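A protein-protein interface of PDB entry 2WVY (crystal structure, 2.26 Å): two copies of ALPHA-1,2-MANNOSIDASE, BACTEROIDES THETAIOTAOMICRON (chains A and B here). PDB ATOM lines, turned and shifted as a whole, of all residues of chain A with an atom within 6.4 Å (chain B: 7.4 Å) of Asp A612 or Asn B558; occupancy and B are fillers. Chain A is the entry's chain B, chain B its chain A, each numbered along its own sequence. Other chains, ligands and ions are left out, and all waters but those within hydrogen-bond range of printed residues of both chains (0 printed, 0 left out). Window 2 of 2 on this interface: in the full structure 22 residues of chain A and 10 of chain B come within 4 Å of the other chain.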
ATOM      1  N   GLU A 282     -13.434  -6.182   6.647  1.00  0.00           N
ATOM      2  CA  GLU A 282     -14.389  -5.956   5.556  1.00  0.00           C
ATOM      3  C   GLU A 282     -14.859  -7.271   4.906  1.00  0.00           C
ATOM      4  O   GLU A 282     -16.040  -7.442   4.608  1.00  0.00           O
ATOM      5  CB  GLU A 282     -13.789  -4.976   4.524  1.00  0.00           C
ATOM      6  CG  GLU A 282     -14.706  -4.607   3.375  1.00  0.00           C
ATOM      7  CD  GLU A 282     -16.022  -3.965   3.828  1.00  0.00           C
ATOM      8  OE1 GLU A 282     -16.062  -3.279   4.870  1.00  0.00           O
ATOM      9  OE2 GLU A 282     -17.033  -4.156   3.123  1.00  0.00           O
ATOM     10  N   GLN A 283     -13.943  -8.207   4.705  1.00  0.00           N
ATOM     11  CA  GLN A 283     -14.315  -9.512   4.173  1.00  0.00           C
ATOM     12  C   GLN A 283     -15.162 -10.288   5.179  1.00  0.00           C
ATOM     13  O   GLN A 283     -16.182 -10.888   4.813  1.00  0.00           O
ATOM     14  CB  GLN A 283     -13.059 -10.309   3.764  1.00  0.00           C
ATOM     15  CG  GLN A 283     -12.258  -9.636   2.655  1.00  0.00           C
ATOM     16  CD  GLN A 283     -10.919 -10.298   2.386  1.00  0.00           C
ATOM     17  OE1 GLN A 283     -10.213 -10.722   3.310  1.00  0.00           O
ATOM     18  NE2 GLN A 283     -10.558 -10.387   1.110  1.00  0.00           N
ATOM     19  N   LEU A 607     -13.353 -15.440 -10.240  1.00  0.00           N
ATOM     20  CA  LEU A 607     -14.045 -15.592  -8.982  1.00  0.00           C
ATOM     21  C   LEU A 607     -13.521 -14.596  -7.937  1.00  0.00           C
ATOM     22  O   LEU A 607     -14.285 -13.872  -7.289  1.00  0.00           O
ATOM     23  CB  LEU A 607     -13.786 -17.016  -8.521  1.00  0.00           C
ATOM     24  CG  LEU A 607     -14.886 -17.851  -7.912  1.00  0.00           C
ATOM     25  CD1 LEU A 607     -14.976 -17.386  -6.458  1.00  0.00           C
ATOM     26  CD2 LEU A 607     -16.215 -17.704  -8.650  1.00  0.00           C
ATOM     27  N   ARG A 608     -12.206 -14.560  -7.773  1.00  0.00           N
ATOM     28  CA  ARG A 608     -11.604 -13.662  -6.799  1.00  0.00           C
ATOM     29  C   ARG A 608     -11.817 -12.218  -7.218  1.00  0.00           C
ATOM     30  O   ARG A 608     -12.086 -11.346  -6.387  1.00  0.00           O
ATOM     31  CB  ARG A 608     -10.122 -13.990  -6.620  1.00  0.00           C
ATOM     32  CG  ARG A 608      -9.888 -15.385  -6.009  1.00  0.00           C
ATOM     33  CD  ARG A 608     -10.333 -15.477  -4.523  1.00  0.00           C
ATOM     34  NE  ARG A 608      -9.527 -14.585  -3.687  1.00  0.00           N
ATOM     35  CZ  ARG A 608      -8.301 -14.874  -3.246  1.00  0.00           C
ATOM     36  NH1 ARG A 608      -7.731 -16.049  -3.523  1.00  0.00           N
ATOM     37  NH2 ARG A 608      -7.643 -13.985  -2.518  1.00  0.00           N
ATOM     38  N   ASN A 609     -11.730 -11.971  -8.515  1.00  0.00           N
ATOM     39  CA  ASN A 609     -12.014 -10.656  -9.048  1.00  0.00           C
ATOM     40  C   ASN A 609     -13.428 -10.192  -8.665  1.00  0.00           C
ATOM     41  O   ASN A 609     -13.621  -9.067  -8.206  1.00  0.00           O
ATOM     42  CB  ASN A 609     -11.844 -10.681 -10.570  1.00  0.00           C
ATOM     43  CG  ASN A 609     -11.423  -9.346 -11.135  1.00  0.00           C
ATOM     44  OD1 ASN A 609     -10.794  -8.535 -10.453  1.00  0.00           O
ATOM     45  ND2 ASN A 609     -11.760  -9.108 -12.399  1.00  0.00           N
ATOM     46  N   VAL A 610     -14.416 -11.064  -8.841  1.00  0.00           N
ATOM     47  CA  VAL A 610     -15.800 -10.707  -8.523  1.00  0.00           C
ATOM     48  C   VAL A 610     -15.996 -10.432  -7.028  1.00  0.00           C
ATOM     49  O   VAL A 610     -16.641  -9.451  -6.658  1.00  0.00           O
ATOM     50  CB  VAL A 610     -16.807 -11.776  -9.013  1.00  0.00           C
ATOM     51  CG1 VAL A 610     -18.169 -11.539  -8.401  1.00  0.00           C
ATOM     52  CG2 VAL A 610     -16.894 -11.755 -10.542  1.00  0.00           C
ATOM     53  N   MET A 611     -15.414 -11.279  -6.182  1.00  0.00           N
ATOM     54  CA  MET A 611     -15.559 -11.110  -4.744  1.00  0.00           C
ATOM     55  C   MET A 611     -14.993  -9.775  -4.268  1.00  0.00           C
ATOM     56  O   MET A 611     -15.610  -9.124  -3.433  1.00  0.00           O
ATOM     57  CB  MET A 611     -14.953 -12.288  -3.959  1.00  0.00           C
ATOM     58  CG  MET A 611     -15.926 -13.456  -3.763  1.00  0.00           C
ATOM     59  SD  MET A 611     -15.285 -14.952  -2.947  1.00  0.00           S
ATOM     60  CE  MET A 611     -14.004 -15.472  -4.073  1.00  0.00           C
ATOM     61  N   ASP A 612     -13.846  -9.386  -4.810  1.00  0.00           N
ATOM     62  CA  ASP A 612     -13.178  -8.138  -4.464  1.00  0.00           C
ATOM     63  C   ASP A 612     -13.885  -6.890  -4.976  1.00  0.00           C
ATOM     64  O   ASP A 612     -13.811  -5.842  -4.356  1.00  0.00           O
ATOM     65  CB  ASP A 612     -11.750  -8.136  -5.033  1.00  0.00           C
ATOM     66  CG  ASP A 612     -10.820  -9.085  -4.285  1.00  0.00           C
ATOM     67  OD1 ASP A 612     -11.221  -9.645  -3.236  1.00  0.00           O
ATOM     68  OD2 ASP A 612      -9.671  -9.253  -4.737  1.00  0.00           O
ATOM     69  N   LYS A 613     -14.540  -6.990  -6.123  1.00  0.00           N
ATOM     70  CA  LYS A 613     -14.990  -5.789  -6.808  1.00  0.00           C
ATOM     71  C   LYS A 613     -16.486  -5.496  -6.740  1.00  0.00           C
ATOM     72  O   LYS A 613     -16.890  -4.339  -6.851  1.00  0.00           O
ATOM     73  CB  LYS A 613     -14.469  -5.799  -8.244  1.00  0.00           C
ATOM     74  CG  LYS A 613     -12.964  -5.546  -8.258  1.00  0.00           C
ATOM     75  CD  LYS A 613     -12.308  -5.965  -9.534  1.00  0.00           C
ATOM     76  CE  LYS A 613     -10.816  -5.610  -9.508  1.00  0.00           C
ATOM     77  NZ  LYS A 613     -10.294  -5.490 -10.912  1.00  0.00           N
ATOM     78  N   LEU A 614     -17.302  -6.526  -6.542  1.00  0.00           N
ATOM     79  CA  LEU A 614     -18.757  -6.341  -6.585  1.00  0.00           C
ATOM     80  C   LEU A 614     -19.424  -6.498  -5.221  1.00  0.00           C
ATOM     81  O   LEU A 614     -20.639  -6.464  -5.109  1.00  0.00           O
ATOM     82  CB  LEU A 614     -19.392  -7.302  -7.599  1.00  0.00           C
ATOM     83  CG  LEU A 614     -18.791  -7.146  -9.003  1.00  0.00           C
ATOM     84  CD1 LEU A 614     -19.463  -8.076  -9.985  1.00  0.00           C
ATOM     85  CD2 LEU A 614     -18.902  -5.711  -9.473  1.00  0.00           C
ATOM     86  N   TYR A 615     -18.622  -6.659  -4.177  1.00  0.00           N
ATOM     87  CA  TYR A 615     -19.170  -6.847  -2.842  1.00  0.00           C
ATOM     88  C   TYR A 615     -18.543  -5.917  -1.835  1.00  0.00           C
ATOM     89  O   TYR A 615     -17.374  -5.550  -1.950  1.00  0.00           O
ATOM     90  CB  TYR A 615     -18.935  -8.274  -2.376  1.00  0.00           C
ATOM     91  CG  TYR A 615     -19.813  -9.279  -3.063  1.00  0.00           C
ATOM     92  CD1 TYR A 615     -21.101  -9.513  -2.612  1.00  0.00           C
ATOM     93  CD2 TYR A 615     -19.366  -9.983  -4.178  1.00  0.00           C
ATOM     94  CE1 TYR A 615     -21.921 -10.428  -3.232  1.00  0.00           C
ATOM     95  CE2 TYR A 615     -20.186 -10.912  -4.809  1.00  0.00           C
ATOM     96  CZ  TYR A 615     -21.462 -11.127  -4.328  1.00  0.00           C
ATOM     97  OH  TYR A 615     -22.305 -12.044  -4.938  1.00  0.00           O
ATOM     98  N   ASN A 616     -19.331  -5.528  -0.846  1.00  0.00           N
ATOM     99  CA  ASN A 616     -18.789  -4.940   0.366  1.00  0.00           C
ATOM    100  C   ASN A 616     -19.867  -5.027   1.438  1.00  0.00           C
ATOM    101  O   ASN A 616     -20.957  -5.514   1.164  1.00  0.00           O
ATOM    102  CB  ASN A 616     -18.260  -3.520   0.140  1.00  0.00           C
ATOM    103  CG  ASN A 616     -19.344  -2.533  -0.256  1.00  0.00           C
ATOM    104  OD1 ASN A 616     -19.247  -1.869  -1.288  1.00  0.00           O
ATOM    105  ND2 ASN A 616     -20.377  -2.430   0.559  1.00  0.00           N
ATOM    106  N   GLY A 621     -23.938  -2.685  -0.386  1.00  0.00           N
ATOM    107  CA  GLY A 621     -23.045  -3.834  -0.461  1.00  0.00           C
ATOM    108  C   GLY A 621     -23.012  -4.659  -1.741  1.00  0.00           C
ATOM    109  O   GLY A 621     -21.957  -5.136  -2.158  1.00  0.00           O
ATOM    110  N   CYS A 623     -22.802  -4.482  -5.248  1.00  0.00           N
ATOM    111  CA  CYS A 623     -22.502  -3.431  -6.248  1.00  0.00           C
ATOM    112  C   CYS A 623     -22.859  -3.849  -7.656  1.00  0.00           C
ATOM    113  O   CYS A 623     -22.899  -3.017  -8.556  1.00  0.00           O
ATOM    114  CB  CYS A 623     -21.005  -3.056  -6.278  1.00  0.00           C
ATOM    115  SG  CYS A 623     -20.195  -2.747  -4.706  1.00  0.00           S
ATOM    116  N   TYR A 635     -21.849 -15.974  -2.713  1.00  0.00           N
ATOM    117  CA  TYR A 635     -20.680 -15.408  -2.060  1.00  0.00           C
ATOM    118  C   TYR A 635     -20.183 -16.321  -0.949  1.00  0.00           C
ATOM    119  O   TYR A 635     -18.967 -16.580  -0.815  1.00  0.00           O
ATOM    120  CB  TYR A 635     -21.000 -14.022  -1.482  1.00  0.00           C
ATOM    121  CG  TYR A 635     -19.801 -13.295  -0.918  1.00  0.00           C
ATOM    122  CD1 TYR A 635     -19.055 -12.422  -1.716  1.00  0.00           C
ATOM    123  CD2 TYR A 635     -19.399 -13.483   0.408  1.00  0.00           C
ATOM    124  CE1 TYR A 635     -17.972 -11.754  -1.212  1.00  0.00           C
ATOM    125  CE2 TYR A 635     -18.312 -12.808   0.924  1.00  0.00           C
ATOM    126  CZ  TYR A 635     -17.595 -11.939   0.105  1.00  0.00           C
ATOM    127  OH  TYR A 635     -16.498 -11.239   0.590  1.00  0.00           O
ATOM    128  N   LEU A 658     -11.573 -17.215  -0.248  1.00  0.00           N
ATOM    129  CA  LEU A 658     -11.286 -15.838   0.090  1.00  0.00           C
ATOM    130  C   LEU A 658     -10.316 -15.720   1.286  1.00  0.00           C
ATOM    131  O   LEU A 658      -9.480 -14.819   1.327  1.00  0.00           O
ATOM    132  CB  LEU A 658     -12.588 -15.083   0.367  1.00  0.00           C
ATOM    133  CG  LEU A 658     -12.506 -13.550   0.418  1.00  0.00           C
ATOM    134  CD1 LEU A 658     -11.903 -12.959  -0.866  1.00  0.00           C
ATOM    135  CD2 LEU A 658     -13.872 -12.982   0.663  1.00  0.00           C
ATOM    136  N   ALA A 681      -4.573 -11.049  -1.538  1.00  0.00           N
ATOM    137  CA  ALA A 681      -5.376 -10.473  -2.614  1.00  0.00           C
ATOM    138  C   ALA A 681      -4.775 -10.707  -3.994  1.00  0.00           C
ATOM    139  O   ALA A 681      -5.503 -10.827  -4.972  1.00  0.00           O
ATOM    140  CB  ALA A 681      -5.597  -8.977  -2.383  1.00  0.00           C
ATOM    141  N   ASN B 555     -21.812   4.537 -10.762  1.00  0.00           N
ATOM    142  CA  ASN B 555     -21.450   3.363  -9.970  1.00  0.00           C
ATOM    143  C   ASN B 555     -19.931   3.223  -9.910  1.00  0.00           C
ATOM    144  O   ASN B 555     -19.294   2.922 -10.908  1.00  0.00           O
ATOM    145  CB  ASN B 555     -22.068   2.100 -10.555  1.00  0.00           C
ATOM    146  CG  ASN B 555     -21.921   0.899  -9.633  1.00  0.00           C
ATOM    147  OD1 ASN B 555     -21.180   0.943  -8.651  1.00  0.00           O
ATOM    148  ND2 ASN B 555     -22.621  -0.183  -9.951  1.00  0.00           N
ATOM    149  N   THR B 556     -19.357   3.447  -8.733  1.00  0.00           N
ATOM    150  CA  THR B 556     -17.916   3.377  -8.559  1.00  0.00           C
ATOM    151  C   THR B 556     -17.465   2.040  -8.020  1.00  0.00           C
ATOM    152  O   THR B 556     -16.271   1.767  -7.990  1.00  0.00           O
ATOM    153  CB  THR B 556     -17.451   4.396  -7.527  1.00  0.00           C
ATOM    154  OG1 THR B 556     -18.347   4.356  -6.412  1.00  0.00           O
ATOM    155  CG2 THR B 556     -17.462   5.805  -8.112  1.00  0.00           C
ATOM    156  N   TYR B 557     -18.410   1.237  -7.547  1.00  0.00           N
ATOM    157  CA  TYR B 557     -18.076  -0.028  -6.916  1.00  0.00           C
ATOM    158  C   TYR B 557     -17.141   0.224  -5.745  1.00  0.00           C
ATOM    159  O   TYR B 557     -17.365   1.130  -4.948  1.00  0.00           O
ATOM    160  CB  TYR B 557     -17.410  -0.957  -7.926  1.00  0.00           C
ATOM    161  CG  TYR B 557     -18.220  -1.103  -9.186  1.00  0.00           C
ATOM    162  CD1 TYR B 557     -19.134  -2.127  -9.317  1.00  0.00           C
ATOM    163  CD2 TYR B 557     -18.092  -0.196 -10.231  1.00  0.00           C
ATOM    164  CE1 TYR B 557     -19.891  -2.270 -10.457  1.00  0.00           C
ATOM    165  CE2 TYR B 557     -18.840  -0.329 -11.386  1.00  0.00           C
ATOM    166  CZ  TYR B 557     -19.746  -1.372 -11.493  1.00  0.00           C
ATOM    167  OH  TYR B 557     -20.519  -1.531 -12.626  1.00  0.00           O
ATOM    168  N   ASN B 558     -16.078  -0.567  -5.663  1.00  0.00           N
ATOM    169  CA  ASN B 558     -15.084  -0.414  -4.604  1.00  0.00           C
ATOM    170  C   ASN B 558     -13.904   0.470  -5.024  1.00  0.00           C
ATOM    171  O   ASN B 558     -12.888   0.538  -4.329  1.00  0.00           O
ATOM    172  CB  ASN B 558     -14.579  -1.789  -4.146  1.00  0.00           C
ATOM    173  CG  ASN B 558     -15.665  -2.628  -3.491  1.00  0.00           C
ATOM    174  OD1 ASN B 558     -16.598  -2.098  -2.896  1.00  0.00           O
ATOM    175  ND2 ASN B 558     -15.541  -3.946  -3.593  1.00  0.00           N
ATOM    176  N   TYR B 559     -14.025   1.142  -6.165  1.00  0.00           N
ATOM    177  CA  TYR B 559     -12.914   1.961  -6.643  1.00  0.00           C
ATOM    178  C   TYR B 559     -12.780   3.327  -5.964  1.00  0.00           C
ATOM    179  O   TYR B 559     -11.742   3.978  -6.079  1.00  0.00           O
ATOM    180  CB  TYR B 559     -12.970   2.112  -8.155  1.00  0.00           C
ATOM    181  CG  TYR B 559     -12.775   0.805  -8.865  1.00  0.00           C
ATOM    182  CD1 TYR B 559     -11.513   0.242  -8.977  1.00  0.00           C
ATOM    183  CD2 TYR B 559     -13.849   0.126  -9.408  1.00  0.00           C
ATOM    184  CE1 TYR B 559     -11.324  -0.953  -9.622  1.00  0.00           C
ATOM    185  CE2 TYR B 559     -13.673  -1.070 -10.060  1.00  0.00           C
ATOM    186  CZ  TYR B 559     -12.408  -1.605 -10.163  1.00  0.00           C
ATOM    187  OH  TYR B 559     -12.220  -2.803 -10.808  1.00  0.00           O
ATOM    188  N   GLY B 560     -13.812   3.774  -5.256  1.00  0.00           N
ATOM    189  CA  GLY B 560     -13.694   5.034  -4.531  1.00  0.00           C
ATOM    190  C   GLY B 560     -12.341   5.137  -3.837  1.00  0.00           C
ATOM    191  O   GLY B 560     -11.808   6.233  -3.638  1.00  0.00           O
ATOM    192  N   THR B 561     -11.788   3.984  -3.466  1.00  0.00           N
ATOM    193  CA  THR B 561     -10.513   3.951  -2.765  1.00  0.00           C
ATOM    194  C   THR B 561      -9.588   4.938  -3.456  1.00  0.00           C
ATOM    195  O   THR B 561      -8.924   5.749  -2.810  1.00  0.00           O
ATOM    196  CB  THR B 561      -9.875   2.543  -2.783  1.00  0.00           C
ATOM    197  N   TYR B 562      -9.560   4.869  -4.782  1.00  0.00           N
ATOM    198  CA  TYR B 562      -8.694   5.741  -5.565  1.00  0.00           C
ATOM    199  C   TYR B 562      -9.061   7.209  -5.315  1.00  0.00           C
ATOM    200  O   TYR B 562      -8.428   8.128  -5.850  1.00  0.00           O
ATOM    201  CB  TYR B 562      -8.777   5.396  -7.058  1.00  0.00           C
ATOM    202  N   ILE B 566     -12.022   9.282  -8.685  1.00  0.00           N
ATOM    203  CA  ILE B 566     -12.783   8.134  -9.165  1.00  0.00           C
ATOM    204  C   ILE B 566     -14.256   8.514  -9.306  1.00  0.00           C
ATOM    205  O   ILE B 566     -14.945   8.055 -10.216  1.00  0.00           O
ATOM    206  CB  ILE B 566     -12.643   6.925  -8.217  1.00  0.00           C
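ND2 of Asn B555 is in hydrogen-bond range of O of Cys A623 (3.2 Å).
ND2 of Asn B558 sits at hydrogen-bond distance from O of Asp A612 (2.7 Å).
The side-chain amino group (NZ) of Lys A613 sits at hydrogen-bond distance from the side-chain hydroxyl (OH) of Tyr B559 (3.3 Å).
OD1 of Asn B558 sits close to OD1 of Asn A616.
The side-chain amide nitrogen (ND2) of Asn B558 is in hydrogen-bond range of the backbone carbonyl oxygen (O) of Tyr A615.
O of Leu A614 is in hydrogen-bond range of N of Cys A623, at 2.9 Å.
OD1 of Asn A609 lies close to NZ of Lys A613 (3.1 Å).
The backbone NH (N) of Asn A616 sits at hydrogen-bond distance from the backbone carbonyl oxygen (O) of Gly A621 (3.0 Å).
SG of Cys A623 lies within hydrogen-bond range of OD1 of Asn A616 (3.7 Å).
OD1 of Asn B555 is in hydrogen-bond range of N of Tyr B557 (3.0 Å).
Lys A613 touches Tyr B557.
O of Lys A613 touches ND2 of Asn B558 (3.5 Å).
CD2 of Leu A614 touches CD1 of Tyr B557, at 3.6 Å.
Cys A623 touches Tyr B557.
Asp A612 touches just one residue of chain B: Asn B558 (2.7 Å).
Of the printed residues of chain B, Tyr A615 touches Asn B558 (2.9 Å).
Of the printed residues of chain B, Asn A616 touches Asn B558 (3.1 Å).
Of the printed residues of chain B, Cys A623 touches Asn B555 (3.2 Å) and Tyr B557 (3.6 Å).
Ala A681 touches none of the printed residues of chain B.
Of the printed residues of chain A, Asn B555 touches Cys A623 (3.2 Å).
Of chain A, only Asp A612 (2.7 Å), Lys A613 (3.5 Å), Tyr A615 (2.9 Å) and Asn A616 (3.1 Å) come within 4 Å of Asn B558.
Of the printed residues of chain A, Tyr B559 touches Lys A613.
Gly B560 touches none of the printed residues of chain A.
The nearest residue of chain B that does not touch Asp A612 is Tyr B557 (7.0 Å).
The nearest residue of chain A that does not touch Asn B558 is Cys A623 (4.1 Å).
The nearest printed residue of chain B that does not touch Tyr A615 is Tyr B557 (6.9 Å).
Printed residues of chain A that touch a printed residue of chain B: Asp A612, Lys A613, Leu A614, Tyr A615, Asn A616 and Cys A623.
Hydrophobic or aromatic side chains of chain A that line the printed part of chain B: Leu A614.
Hydrophobic or aromatic side chains of chain B that line the printed part of chain A: Tyr B557 and Tyr B559.
Among the printed residues, no Asp or Glu carboxylate lies within 4 Å of a Lys or Arg side-chain nitrogen of the other chain.
No position is printed for both chains.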
